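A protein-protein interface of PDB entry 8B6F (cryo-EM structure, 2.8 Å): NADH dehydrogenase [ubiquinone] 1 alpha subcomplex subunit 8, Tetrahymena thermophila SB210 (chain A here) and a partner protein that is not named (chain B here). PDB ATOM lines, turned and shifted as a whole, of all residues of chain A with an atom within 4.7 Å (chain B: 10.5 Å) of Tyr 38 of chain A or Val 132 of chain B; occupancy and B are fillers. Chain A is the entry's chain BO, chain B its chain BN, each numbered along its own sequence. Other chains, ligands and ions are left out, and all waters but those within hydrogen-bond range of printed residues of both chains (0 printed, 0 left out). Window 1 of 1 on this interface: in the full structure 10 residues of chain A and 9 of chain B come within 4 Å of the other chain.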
ATOM      1  N   CYS A  35      -9.539 -16.760 -26.689  1.00  0.00           N
ATOM      2  CA  CYS A  35     -10.820 -16.127 -26.400  1.00  0.00           C
ATOM      3  C   CYS A  35     -11.183 -16.159 -24.921  1.00  0.00           C
ATOM      4  O   CYS A  35     -12.324 -15.844 -24.570  1.00  0.00           O
ATOM      5  CB  CYS A  35     -11.931 -16.800 -27.211  1.00  0.00           C
ATOM      6  SG  CYS A  35     -11.482 -17.237 -28.905  1.00  0.00           S
ATOM      7  N   GLY A  36     -10.250 -16.528 -24.045  1.00  0.00           N
ATOM      8  CA  GLY A  36     -10.561 -16.577 -22.627  1.00  0.00           C
ATOM      9  C   GLY A  36     -11.017 -15.253 -22.055  1.00  0.00           C
ATOM     10  O   GLY A  36     -11.703 -15.234 -21.028  1.00  0.00           O
ATOM     11  N   TYR A  37     -10.652 -14.143 -22.694  1.00  0.00           N
ATOM     12  CA  TYR A  37     -11.103 -12.836 -22.229  1.00  0.00           C
ATOM     13  C   TYR A  37     -12.620 -12.735 -22.263  1.00  0.00           C
ATOM     14  O   TYR A  37     -13.237 -12.177 -21.349  1.00  0.00           O
ATOM     15  CB  TYR A  37     -10.466 -11.744 -23.087  1.00  0.00           C
ATOM     16  CG  TYR A  37     -10.926 -10.344 -22.770  1.00  0.00           C
ATOM     17  CD1 TYR A  37     -10.367  -9.633 -21.719  1.00  0.00           C
ATOM     18  CD2 TYR A  37     -11.900  -9.724 -23.537  1.00  0.00           C
ATOM     19  CE1 TYR A  37     -10.776  -8.350 -21.430  1.00  0.00           C
ATOM     20  CE2 TYR A  37     -12.316  -8.440 -23.258  1.00  0.00           C
ATOM     21  CZ  TYR A  37     -11.748  -7.758 -22.204  1.00  0.00           C
ATOM     22  OH  TYR A  37     -12.157  -6.481 -21.920  1.00  0.00           O
ATOM     23  N   TYR A  38     -13.241 -13.268 -23.316  1.00  0.00           N
ATOM     24  CA  TYR A  38     -14.688 -13.164 -23.459  1.00  0.00           C
ATOM     25  C   TYR A  38     -15.419 -13.931 -22.365  1.00  0.00           C
ATOM     26  O   TYR A  38     -16.467 -13.489 -21.885  1.00  0.00           O
ATOM     27  CB  TYR A  38     -15.107 -13.671 -24.837  1.00  0.00           C
ATOM     28  CG  TYR A  38     -14.617 -12.814 -25.981  1.00  0.00           C
ATOM     29  CD1 TYR A  38     -14.697 -11.428 -25.923  1.00  0.00           C
ATOM     30  CD2 TYR A  38     -14.070 -13.392 -27.117  1.00  0.00           C
ATOM     31  CE1 TYR A  38     -14.252 -10.644 -26.964  1.00  0.00           C
ATOM     32  CE2 TYR A  38     -13.621 -12.615 -28.165  1.00  0.00           C
ATOM     33  CZ  TYR A  38     -13.714 -11.241 -28.083  1.00  0.00           C
ATOM     34  OH  TYR A  38     -13.267 -10.464 -29.125  1.00  0.00           O
ATOM     35  N   LEU A  39     -14.883 -15.082 -21.955  1.00  0.00           N
ATOM     36  CA  LEU A  39     -15.550 -15.874 -20.927  1.00  0.00           C
ATOM     37  C   LEU A  39     -15.501 -15.170 -19.577  1.00  0.00           C
ATOM     38  O   LEU A  39     -16.509 -15.114 -18.864  1.00  0.00           O
ATOM     39  CB  LEU A  39     -14.914 -17.260 -20.837  1.00  0.00           C
ATOM     40  CG  LEU A  39     -15.689 -18.320 -20.049  1.00  0.00           C
ATOM     41  CD1 LEU A  39     -17.040 -18.614 -20.687  1.00  0.00           C
ATOM     42  CD2 LEU A  39     -14.870 -19.588 -19.932  1.00  0.00           C
ATOM     43  N   GLN A  40     -14.342 -14.628 -19.208  1.00  0.00           N
ATOM     44  CA  GLN A  40     -14.256 -13.839 -17.986  1.00  0.00           C
ATOM     45  C   GLN A  40     -15.172 -12.627 -18.069  1.00  0.00           C
ATOM     46  O   GLN A  40     -15.813 -12.252 -17.081  1.00  0.00           O
ATOM     47  CB  GLN A  40     -12.812 -13.407 -17.736  1.00  0.00           C
ATOM     48  CG  GLN A  40     -12.573 -12.841 -16.345  1.00  0.00           C
ATOM     49  CD  GLN A  40     -12.640 -13.896 -15.261  1.00  0.00           C
ATOM     50  OE1 GLN A  40     -13.364 -13.747 -14.279  1.00  0.00           O
ATOM     51  NE2 GLN A  40     -11.878 -14.970 -15.431  1.00  0.00           N
ATOM     52  N   GLY A  41     -15.247 -12.006 -19.244  1.00  0.00           N
ATOM     53  CA  GLY A  41     -16.180 -10.910 -19.435  1.00  0.00           C
ATOM     54  C   GLY A  41     -17.621 -11.330 -19.232  1.00  0.00           C
ATOM     55  O   GLY A  41     -18.420 -10.586 -18.660  1.00  0.00           O
ATOM     56  N   ILE A  42     -17.978 -12.523 -19.707  1.00  0.00           N
ATOM     57  CA  ILE A  42     -19.339 -13.012 -19.516  1.00  0.00           C
ATOM     58  C   ILE A  42     -19.640 -13.169 -18.033  1.00  0.00           C
ATOM     59  O   ILE A  42     -20.713 -12.780 -17.558  1.00  0.00           O
ATOM     60  CB  ILE A  42     -19.538 -14.334 -20.284  1.00  0.00           C
ATOM     61  CG1 ILE A  42     -19.573 -14.067 -21.790  1.00  0.00           C
ATOM     62  CG2 ILE A  42     -20.826 -15.026 -19.849  1.00  0.00           C
ATOM     63  CD1 ILE A  42     -19.472 -15.318 -22.637  1.00  0.00           C
ATOM     64  N   ARG A  70     -23.880  -9.341 -26.454  1.00  0.00           N
ATOM     65  CA  ARG A  70     -22.727  -8.993 -27.277  1.00  0.00           C
ATOM     66  C   ARG A  70     -21.507  -9.814 -26.882  1.00  0.00           C
ATOM     67  O   ARG A  70     -20.749 -10.267 -27.747  1.00  0.00           O
ATOM     68  CB  ARG A  70     -22.431  -7.498 -27.172  1.00  0.00           C
ATOM     69  CG  ARG A  70     -23.600  -6.620 -27.588  1.00  0.00           C
ATOM     70  CD  ARG A  70     -23.159  -5.202 -27.915  1.00  0.00           C
ATOM     71  NE  ARG A  70     -22.347  -4.612 -26.855  1.00  0.00           N
ATOM     72  CZ  ARG A  70     -21.021  -4.553 -26.858  1.00  0.00           C
ATOM     73  NH1 ARG A  70     -20.306  -5.044 -27.858  1.00  0.00           N
ATOM     74  NH2 ARG A  70     -20.396  -3.986 -25.831  1.00  0.00           N
ATOM     75  N   LEU A  71     -21.286  -9.999 -25.579  1.00  0.00           N
ATOM     76  CA  LEU A  71     -20.162 -10.817 -25.134  1.00  0.00           C
ATOM     77  C   LEU A  71     -20.312 -12.261 -25.594  1.00  0.00           C
ATOM     78  O   LEU A  71     -19.343 -12.877 -26.053  1.00  0.00           O
ATOM     79  CB  LEU A  71     -20.041 -10.755 -23.612  1.00  0.00           C
ATOM     80  CG  LEU A  71     -19.416  -9.481 -23.046  1.00  0.00           C
ATOM     81  CD1 LEU A  71     -19.676  -9.383 -21.555  1.00  0.00           C
ATOM     82  CD2 LEU A  71     -17.926  -9.447 -23.331  1.00  0.00           C
ATOM     83  N   ALA A  74     -19.638 -12.442 -29.324  1.00  0.00           N
ATOM     84  CA  ALA A  74     -18.212 -12.295 -29.591  1.00  0.00           C
ATOM     85  C   ALA A  74     -17.457 -13.568 -29.241  1.00  0.00           C
ATOM     86  O   ALA A  74     -16.567 -13.995 -29.985  1.00  0.00           O
ATOM     87  CB  ALA A  74     -17.652 -11.111 -28.808  1.00  0.00           C
ATOM     88  N   HIS A  75     -17.800 -14.191 -28.113  1.00  0.00           N
ATOM     89  CA  HIS A  75     -17.143 -15.437 -27.739  1.00  0.00           C
ATOM     90  C   HIS A  75     -17.423 -16.526 -28.763  1.00  0.00           C
ATOM     91  O   HIS A  75     -16.519 -17.278 -29.143  1.00  0.00           O
ATOM     92  CB  HIS A  75     -17.599 -15.876 -26.349  1.00  0.00           C
ATOM     93  CG  HIS A  75     -16.763 -16.965 -25.756  1.00  0.00           C
ATOM     94  ND1 HIS A  75     -15.386 -16.940 -25.775  1.00  0.00           N
ATOM     95  CD2 HIS A  75     -17.108 -18.107 -25.119  1.00  0.00           C
ATOM     96  CE1 HIS A  75     -14.917 -18.021 -25.180  1.00  0.00           C
ATOM     97  NE2 HIS A  75     -15.942 -18.748 -24.772  1.00  0.00           N
ATOM     98  N   CYS A  78     -15.353 -15.818 -31.861  1.00  0.00           N
ATOM     99  CA  CYS A  78     -13.942 -16.099 -31.617  1.00  0.00           C
ATOM    100  C   CYS A  78     -13.674 -17.598 -31.599  1.00  0.00           C
ATOM    101  O   CYS A  78     -12.679 -18.066 -32.164  1.00  0.00           O
ATOM    102  CB  CYS A  78     -13.510 -15.457 -30.298  1.00  0.00           C
ATOM    103  SG  CYS A  78     -11.736 -15.523 -29.961  1.00  0.00           S
ATOM    104  N   GLN B 105      -7.339   1.442 -23.843  1.00  0.00           N
ATOM    105  CA  GLN B 105      -8.437   1.121 -24.744  1.00  0.00           C
ATOM    106  C   GLN B 105      -9.179   2.354 -25.236  1.00  0.00           C
ATOM    107  O   GLN B 105     -10.211   2.213 -25.897  1.00  0.00           O
ATOM    108  CB  GLN B 105      -9.427   0.186 -24.051  1.00  0.00           C
ATOM    109  CG  GLN B 105      -8.843  -1.147 -23.684  1.00  0.00           C
ATOM    110  CD  GLN B 105      -9.754  -1.960 -22.796  1.00  0.00           C
ATOM    111  OE1 GLN B 105     -10.904  -1.593 -22.564  1.00  0.00           O
ATOM    112  NE2 GLN B 105      -9.242  -3.078 -22.293  1.00  0.00           N
ATOM    113  N   LYS B 107      -9.196   4.506 -27.686  1.00  0.00           N
ATOM    114  CA  LYS B 107      -9.722   4.535 -29.047  1.00  0.00           C
ATOM    115  C   LYS B 107     -10.635   3.348 -29.317  1.00  0.00           C
ATOM    116  O   LYS B 107     -11.630   3.475 -30.039  1.00  0.00           O
ATOM    117  CB  LYS B 107      -8.576   4.570 -30.056  1.00  0.00           C
ATOM    118  CG  LYS B 107      -8.963   5.207 -31.381  1.00  0.00           C
ATOM    119  CD  LYS B 107      -7.833   5.133 -32.392  1.00  0.00           C
ATOM    120  CE  LYS B 107      -7.918   3.876 -33.242  1.00  0.00           C
ATOM    121  NZ  LYS B 107      -9.076   3.916 -34.177  1.00  0.00           N
ATOM    122  N   PHE B 108     -10.309   2.179 -28.764  1.00  0.00           N
ATOM    123  CA  PHE B 108     -11.169   1.017 -28.951  1.00  0.00           C
ATOM    124  C   PHE B 108     -12.563   1.254 -28.388  1.00  0.00           C
ATOM    125  O   PHE B 108     -13.539   0.686 -28.891  1.00  0.00           O
ATOM    126  CB  PHE B 108     -10.536  -0.215 -28.306  1.00  0.00           C
ATOM    127  CG  PHE B 108      -9.191  -0.577 -28.874  1.00  0.00           C
ATOM    128  CD1 PHE B 108      -8.880  -0.302 -30.197  1.00  0.00           C
ATOM    129  CD2 PHE B 108      -8.238  -1.193 -28.082  1.00  0.00           C
ATOM    130  CE1 PHE B 108      -7.643  -0.635 -30.716  1.00  0.00           C
ATOM    131  CE2 PHE B 108      -7.001  -1.529 -28.595  1.00  0.00           C
ATOM    132  CZ  PHE B 108      -6.703  -1.249 -29.915  1.00  0.00           C
ATOM    133  N   ILE B 109     -12.680   2.084 -27.350  1.00  0.00           N
ATOM    134  CA  ILE B 109     -13.994   2.388 -26.790  1.00  0.00           C
ATOM    135  C   ILE B 109     -14.858   3.096 -27.823  1.00  0.00           C
ATOM    136  O   ILE B 109     -16.025   2.744 -28.027  1.00  0.00           O
ATOM    137  CB  ILE B 109     -13.853   3.224 -25.503  1.00  0.00           C
ATOM    138  CG1 ILE B 109     -13.094   2.447 -24.420  1.00  0.00           C
ATOM    139  CG2 ILE B 109     -15.224   3.650 -24.983  1.00  0.00           C
ATOM    140  CD1 ILE B 109     -13.769   1.174 -23.957  1.00  0.00           C
ATOM    141  N   GLN B 110     -14.302   4.108 -28.493  1.00  0.00           N
ATOM    142  CA  GLN B 110     -15.089   4.819 -29.494  1.00  0.00           C
ATOM    143  C   GLN B 110     -15.364   3.944 -30.709  1.00  0.00           C
ATOM    144  O   GLN B 110     -16.438   4.043 -31.310  1.00  0.00           O
ATOM    145  CB  GLN B 110     -14.388   6.116 -29.907  1.00  0.00           C
ATOM    146  CG  GLN B 110     -13.053   5.934 -30.607  1.00  0.00           C
ATOM    147  CD  GLN B 110     -12.585   7.202 -31.287  1.00  0.00           C
ATOM    148  OE1 GLN B 110     -13.167   8.270 -31.103  1.00  0.00           O
ATOM    149  NE2 GLN B 110     -11.526   7.091 -32.082  1.00  0.00           N
ATOM    150  N   LEU B 111     -14.415   3.085 -31.086  1.00  0.00           N
ATOM    151  CA  LEU B 111     -14.668   2.151 -32.177  1.00  0.00           C
ATOM    152  C   LEU B 111     -15.827   1.226 -31.836  1.00  0.00           C
ATOM    153  O   LEU B 111     -16.700   0.972 -32.673  1.00  0.00           O
ATOM    154  CB  LEU B 111     -13.408   1.344 -32.484  1.00  0.00           C
ATOM    155  CG  LEU B 111     -12.266   2.094 -33.171  1.00  0.00           C
ATOM    156  CD1 LEU B 111     -11.033   1.211 -33.251  1.00  0.00           C
ATOM    157  CD2 LEU B 111     -12.672   2.564 -34.556  1.00  0.00           C
ATOM    158  N   GLU B 112     -15.852   0.713 -30.604  1.00  0.00           N
ATOM    159  CA  GLU B 112     -16.949  -0.151 -30.185  1.00  0.00           C
ATOM    160  C   GLU B 112     -18.266   0.612 -30.158  1.00  0.00           C
ATOM    161  O   GLU B 112     -19.311   0.072 -30.537  1.00  0.00           O
ATOM    162  CB  GLU B 112     -16.644  -0.743 -28.809  1.00  0.00           C
ATOM    163  CG  GLU B 112     -17.691  -1.724 -28.309  1.00  0.00           C
ATOM    164  CD  GLU B 112     -17.381  -2.240 -26.918  1.00  0.00           C
ATOM    165  OE1 GLU B 112     -16.384  -1.781 -26.323  1.00  0.00           O
ATOM    166  OE2 GLU B 112     -18.134  -3.103 -26.418  1.00  0.00           O
ATOM    167  N   LYS B 113     -18.239   1.868 -29.709  1.00  0.00           N
ATOM    168  CA  LYS B 113     -19.453   2.675 -29.700  1.00  0.00           C
ATOM    169  C   LYS B 113     -19.990   2.862 -31.113  1.00  0.00           C
ATOM    170  O   LYS B 113     -21.193   2.721 -31.358  1.00  0.00           O
ATOM    171  CB  LYS B 113     -19.176   4.028 -29.044  1.00  0.00           C
ATOM    172  CG  LYS B 113     -20.408   4.916 -28.922  1.00  0.00           C
ATOM    173  CD  LYS B 113     -20.070   6.249 -28.277  1.00  0.00           C
ATOM    174  CE  LYS B 113     -21.304   7.133 -28.166  1.00  0.00           C
ATOM    175  NZ  LYS B 113     -20.993   8.451 -27.544  1.00  0.00           N
ATOM    176  N   HIS B 115     -19.428   0.900 -33.670  1.00  0.00           N
ATOM    177  CA  HIS B 115     -19.917  -0.396 -34.129  1.00  0.00           C
ATOM    178  C   HIS B 115     -21.312  -0.675 -33.587  1.00  0.00           C
ATOM    179  O   HIS B 115     -22.176  -1.186 -34.308  1.00  0.00           O
ATOM    180  CB  HIS B 115     -18.943  -1.497 -33.708  1.00  0.00           C
ATOM    181  CG  HIS B 115     -19.305  -2.854 -34.221  1.00  0.00           C
ATOM    182  ND1 HIS B 115     -20.201  -3.682 -33.579  1.00  0.00           N
ATOM    183  CD2 HIS B 115     -18.886  -3.533 -35.315  1.00  0.00           C
ATOM    184  CE1 HIS B 115     -20.321  -4.809 -34.256  1.00  0.00           C
ATOM    185  NE2 HIS B 115     -19.533  -4.745 -35.315  1.00  0.00           N
ATOM    186  N   ILE B 116     -21.553  -0.349 -32.315  1.00  0.00           N
ATOM    187  CA  ILE B 116     -22.873  -0.565 -31.731  1.00  0.00           C
ATOM    188  C   ILE B 116     -23.909   0.317 -32.414  1.00  0.00           C
ATOM    189  O   ILE B 116     -25.022  -0.129 -32.714  1.00  0.00           O
ATOM    190  CB  ILE B 116     -22.829  -0.318 -30.212  1.00  0.00           C
ATOM    191  CG1 ILE B 116     -21.954  -1.371 -29.531  1.00  0.00           C
ATOM    192  CG2 ILE B 116     -24.234  -0.342 -29.620  1.00  0.00           C
ATOM    193  CD1 ILE B 116     -21.628  -1.060 -28.088  1.00  0.00           C
ATOM    194  N   SER B 119     -24.627  -1.158 -35.746  1.00  0.00           N
ATOM    195  CA  SER B 119     -25.390  -2.392 -35.588  1.00  0.00           C
ATOM    196  C   SER B 119     -26.858  -2.096 -35.309  1.00  0.00           C
ATOM    197  O   SER B 119     -27.746  -2.765 -35.848  1.00  0.00           O
ATOM    198  CB  SER B 119     -24.789  -3.239 -34.467  1.00  0.00           C
ATOM    199  OG  SER B 119     -25.507  -4.449 -34.300  1.00  0.00           O
ATOM    200  N   PHE B 124     -23.727  -3.402 -40.726  1.00  0.00           N
ATOM    201  CA  PHE B 124     -22.999  -4.294 -39.832  1.00  0.00           C
ATOM    202  C   PHE B 124     -21.531  -4.277 -40.233  1.00  0.00           C
ATOM    203  O   PHE B 124     -21.189  -4.680 -41.349  1.00  0.00           O
ATOM    204  CB  PHE B 124     -23.556  -5.718 -39.888  1.00  0.00           C
ATOM    205  CG  PHE B 124     -22.741  -6.715 -39.117  1.00  0.00           C
ATOM    206  CD1 PHE B 124     -22.937  -6.885 -37.756  1.00  0.00           C
ATOM    207  CD2 PHE B 124     -21.779  -7.483 -39.754  1.00  0.00           C
ATOM    208  CE1 PHE B 124     -22.189  -7.802 -37.045  1.00  0.00           C
ATOM    209  CE2 PHE B 124     -21.027  -8.402 -39.048  1.00  0.00           C
ATOM    210  CZ  PHE B 124     -21.231  -8.560 -37.692  1.00  0.00           C
ATOM    211  N   VAL B 125     -20.672  -3.819 -39.329  1.00  0.00           N
ATOM    212  CA  VAL B 125     -19.244  -3.686 -39.593  1.00  0.00           C
ATOM    213  C   VAL B 125     -18.532  -4.885 -38.983  1.00  0.00           C
ATOM    214  O   VAL B 125     -18.585  -5.097 -37.766  1.00  0.00           O
ATOM    215  CB  VAL B 125     -18.688  -2.369 -39.032  1.00  0.00           C
ATOM    216  CG1 VAL B 125     -17.231  -2.191 -39.431  1.00  0.00           C
ATOM    217  CG2 VAL B 125     -19.520  -1.193 -39.512  1.00  0.00           C
ATOM    218  N   GLU B 126     -17.858  -5.665 -39.825  1.00  0.00           N
ATOM    219  CA  GLU B 126     -17.133  -6.841 -39.365  1.00  0.00           C
ATOM    220  C   GLU B 126     -15.711  -6.529 -38.925  1.00  0.00           C
ATOM    221  O   GLU B 126     -15.123  -7.317 -38.177  1.00  0.00           O
ATOM    222  CB  GLU B 126     -17.094  -7.897 -40.475  1.00  0.00           C
ATOM    223  CG  GLU B 126     -16.486  -9.223 -40.049  1.00  0.00           C
ATOM    224  CD  GLU B 126     -16.503 -10.253 -41.161  1.00  0.00           C
ATOM    225  OE1 GLU B 126     -16.808  -9.876 -42.312  1.00  0.00           O
ATOM    226  OE2 GLU B 126     -16.213 -11.436 -40.885  1.00  0.00           O
ATOM    227  N   THR B 127     -15.147  -5.403 -39.364  1.00  0.00           N
ATOM    228  CA  THR B 127     -13.760  -5.094 -39.033  1.00  0.00           C
ATOM    229  C   THR B 127     -13.573  -4.918 -37.532  1.00  0.00           C
ATOM    230  O   THR B 127     -12.596  -5.413 -36.959  1.00  0.00           O
ATOM    231  CB  THR B 127     -13.311  -3.835 -39.773  1.00  0.00           C
ATOM    232  OG1 THR B 127     -14.069  -2.709 -39.312  1.00  0.00           O
ATOM    233  CG2 THR B 127     -13.518  -3.997 -41.267  1.00  0.00           C
ATOM    234  N   THR B 128     -14.497  -4.216 -36.878  1.00  0.00           N
ATOM    235  CA  THR B 128     -14.392  -3.910 -35.459  1.00  0.00           C
ATOM    236  C   THR B 128     -15.215  -4.850 -34.592  1.00  0.00           C
ATOM    237  O   THR B 128     -15.361  -4.600 -33.392  1.00  0.00           O
ATOM    238  CB  THR B 128     -14.822  -2.463 -35.201  1.00  0.00           C
ATOM    239  OG1 THR B 128     -16.146  -2.254 -35.710  1.00  0.00           O
ATOM    240  CG2 THR B 128     -13.864  -1.492 -35.869  1.00  0.00           C
ATOM    241  N   SER B 129     -15.759  -5.922 -35.166  1.00  0.00           N
ATOM    242  CA  SER B 129     -16.575  -6.840 -34.378  1.00  0.00           C
ATOM    243  C   SER B 129     -15.837  -7.412 -33.174  1.00  0.00           C
ATOM    244  O   SER B 129     -16.460  -7.524 -32.104  1.00  0.00           O
ATOM    245  CB  SER B 129     -17.110  -7.963 -35.277  1.00  0.00           C
ATOM    246  OG  SER B 129     -16.072  -8.623 -35.976  1.00  0.00           O
ATOM    247  N   PRO B 130     -14.558  -7.790 -33.256  1.00  0.00           N
ATOM    248  CA  PRO B 130     -13.905  -8.392 -32.082  1.00  0.00           C
ATOM    249  C   PRO B 130     -13.855  -7.475 -30.873  1.00  0.00           C
ATOM    250  O   PRO B 130     -13.733  -7.970 -29.747  1.00  0.00           O
ATOM    251  CB  PRO B 130     -12.494  -8.724 -32.591  1.00  0.00           C
ATOM    252  CG  PRO B 130     -12.594  -8.709 -34.073  1.00  0.00           C
ATOM    253  CD  PRO B 130     -13.624  -7.681 -34.391  1.00  0.00           C
ATOM    254  N   LEU B 131     -13.944  -6.159 -31.064  1.00  0.00           N
ATOM    255  CA  LEU B 131     -13.784  -5.198 -29.973  1.00  0.00           C
ATOM    256  C   LEU B 131     -15.044  -5.195 -29.113  1.00  0.00           C
ATOM    257  O   LEU B 131     -15.951  -4.374 -29.271  1.00  0.00           O
ATOM    258  CB  LEU B 131     -13.478  -3.811 -30.522  1.00  0.00           C
ATOM    259  CG  LEU B 131     -12.123  -3.648 -31.214  1.00  0.00           C
ATOM    260  CD1 LEU B 131     -12.014  -2.274 -31.845  1.00  0.00           C
ATOM    261  CD2 LEU B 131     -10.981  -3.873 -30.237  1.00  0.00           C
ATOM    262  N   VAL B 132     -15.093  -6.139 -28.183  1.00  0.00           N
ATOM    263  CA  VAL B 132     -16.138  -6.203 -27.163  1.00  0.00           C
ATOM    264  C   VAL B 132     -15.416  -6.183 -25.821  1.00  0.00           C
ATOM    265  O   VAL B 132     -14.996  -7.218 -25.301  1.00  0.00           O
ATOM    266  CB  VAL B 132     -17.032  -7.436 -27.312  1.00  0.00           C
ATOM    267  CG1 VAL B 132     -18.130  -7.429 -26.263  1.00  0.00           C
ATOM    268  CG2 VAL B 132     -17.633  -7.476 -28.704  1.00  0.00           C
ATOM    269  N   LEU B 133     -15.276  -4.992 -25.250  1.00  0.00           N
ATOM    270  CA  LEU B 133     -14.470  -4.778 -24.058  1.00  0.00           C
ATOM    271  C   LEU B 133     -15.363  -4.600 -22.839  1.00  0.00           C
ATOM    272  O   LEU B 133     -16.421  -3.969 -22.916  1.00  0.00           O
ATOM    273  CB  LEU B 133     -13.580  -3.547 -24.232  1.00  0.00           C
ATOM    274  CG  LEU B 133     -12.738  -3.521 -25.510  1.00  0.00           C
ATOM    275  CD1 LEU B 133     -12.091  -2.162 -25.693  1.00  0.00           C
ATOM    276  CD2 LEU B 133     -11.684  -4.614 -25.484  1.00  0.00           C
ATOM    277  N   TRP B 134     -14.928  -5.165 -21.709  1.00  0.00           N
ATOM    278  CA  TRP B 134     -15.651  -5.047 -20.451  1.00  0.00           C
ATOM    279  C   TRP B 134     -14.781  -4.495 -19.328  1.00  0.00           C
ATOM    280  O   TRP B 134     -15.227  -4.462 -18.176  1.00  0.00           O
ATOM    281  CB  TRP B 134     -16.222  -6.407 -20.033  1.00  0.00           C
ATOM    282  CG  TRP B 134     -15.178  -7.467 -19.900  1.00  0.00           C
ATOM    283  CD1 TRP B 134     -14.746  -8.313 -20.875  1.00  0.00           C
ATOM    284  CD2 TRP B 134     -14.432  -7.793 -18.722  1.00  0.00           C
ATOM    285  NE1 TRP B 134     -13.775  -9.148 -20.378  1.00  0.00           N
ATOM    286  CE2 TRP B 134     -13.563  -8.848 -19.059  1.00  0.00           C
ATOM    287  CE3 TRP B 134     -14.413  -7.294 -17.417  1.00  0.00           C
ATOM    288  CZ2 TRP B 134     -12.686  -9.415 -18.139  1.00  0.00           C
ATOM    289  CZ3 TRP B 134     -13.540  -7.857 -16.503  1.00  0.00           C
ATOM    290  CH2 TRP B 134     -12.687  -8.907 -16.869  1.00  0.00           C
ATOM    291  N   ASN B 135     -13.561  -4.059 -19.626  1.00  0.00           N
ATOM    292  CA  ASN B 135     -12.670  -3.522 -18.604  1.00  0.00           C
ATOM    293  C   ASN B 135     -11.603  -2.623 -19.219  1.00  0.00           C
ATOM    294  O   ASN B 135     -11.146  -2.856 -20.336  1.00  0.00           O
ATOM    295  CB  ASN B 135     -12.006  -4.654 -17.823  1.00  0.00           C
ATOM    296  CG  ASN B 135     -11.263  -5.620 -18.723  1.00  0.00           C
ATOM    297  OD1 ASN B 135     -11.056  -5.354 -19.905  1.00  0.00           O
ATOM    298  ND2 ASN B 135     -10.853  -6.750 -18.162  1.00  0.00           N
ATOM    299  OXT ASN B 135     -11.164  -1.648 -18.609  1.00  0.00           O
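The side-chain carboxylate (OE2) of Glu 112 of chain B is in salt-bridge range of the guanidinium group (NH2) of Arg 70 of chain A, at 2.5 Å. OH of Tyr 38 of chain A lies within hydrogen-bond range of O of Pro 130 of chain B (2.6 Å). The backbone NH (N) of Trp 134 of chain B lies within hydrogen-bond range of the side-chain hydroxyl (OH) of Tyr 37 of chain A (3.1 Å). The side-chain amide oxygen (OD1) of Asn 135 of chain B sits at hydrogen-bond distance from the side-chain hydroxyl (OH) of Tyr 37 of chain A (2.6 Å). N of Gly 41 of chain A lies close to NE1 of Trp 134 of chain B (3.4 Å).
No residue of chain B comes within 4 Å of Cys 35 of chain A. No residue of chain B comes within 4 Å of Gly 36 of chain A. Tyr 37 of chain A touches four residues of chain B. Of the printed residues of chain B, Tyr 38 of chain A touches Pro 130 (2.6 Å) and Val 132 (3.9 Å). Leu 39 of chain A touches none of the printed residues of chain B. Gly 41 of chain A touches just one residue of chain B: Trp 134. Arg 70 of chain A touches just these residues of chain B: Glu 112, Ile 116 and Val 132. Leu 71 of chain A touches just one residue of chain B: Val 132 (3.6 Å). Ile 109 of chain B touches none of the printed residues of chain A. Printed residues of chain A within 4 Å of Pro 130 of chain B: Tyr 38. Val 132 of chain B touches just these residues of chain A: Tyr 37 (3.6 Å), Tyr 38 (3.9 Å), Arg 70 (3.6 Å), Leu 71 (3.6 Å) and Ala 74 (3.6 Å). Of the printed residues of chain A, Leu 133 of chain B touches Tyr 37 (3.6 Å). Of the printed residues of chain A, Trp 134 of chain B touches Tyr 37 (3.1 Å), Gln 40 (3.9 Å) and Gly 41 (3.1 Å). Of the printed residues of chain A, Asn 135 of chain B touches Tyr 37. The nearest printed residue of chain A that does not touch Ile 116 of chain B is Leu 71 of chain A (9.3 Å).
CE2 of Tyr 37 of chain A touches O of Val 132 of chain B (3.6 Å). Leu 133 of chain B touches Tyr 37 of chain A. CE1 of Tyr 38 of chain A touches O of Val 132 of chain B, at 3.9 Å. Trp 134 of chain B touches Gln 40 of chain A. Arg 70 of chain A touches Ile 116 of chain B (CZ to CD1, 3.8 Å). NH1 of Arg 70 of chain A touches CG1 of Val 132 of chain B (3.6 Å). Val 132 of chain B touches Leu 71 of chain A (CG1 to CD2, 3.6 Å). Ala 74 of chain A touches Val 132 of chain B.
Printed residues of chain A that touch a printed residue of chain B: Tyr 37, Tyr 38, Gln 40, Gly 41, Arg 70, Leu 71 and Ala 74. Hydrophobic or aromatic side chains of chain A within 4 Å of the printed part of chain B: Tyr 37, Tyr 38, Leu 71 and Ala 74.
The chain-end carboxylate (O) of Asn 135 of chain B lies close to the side-chain amide oxygen (OE1) of Gln 105 of chain B. SG of Cys 35 of chain A is disulfide-bonded to SG of Cys 78 of chain A (2.0 Å).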
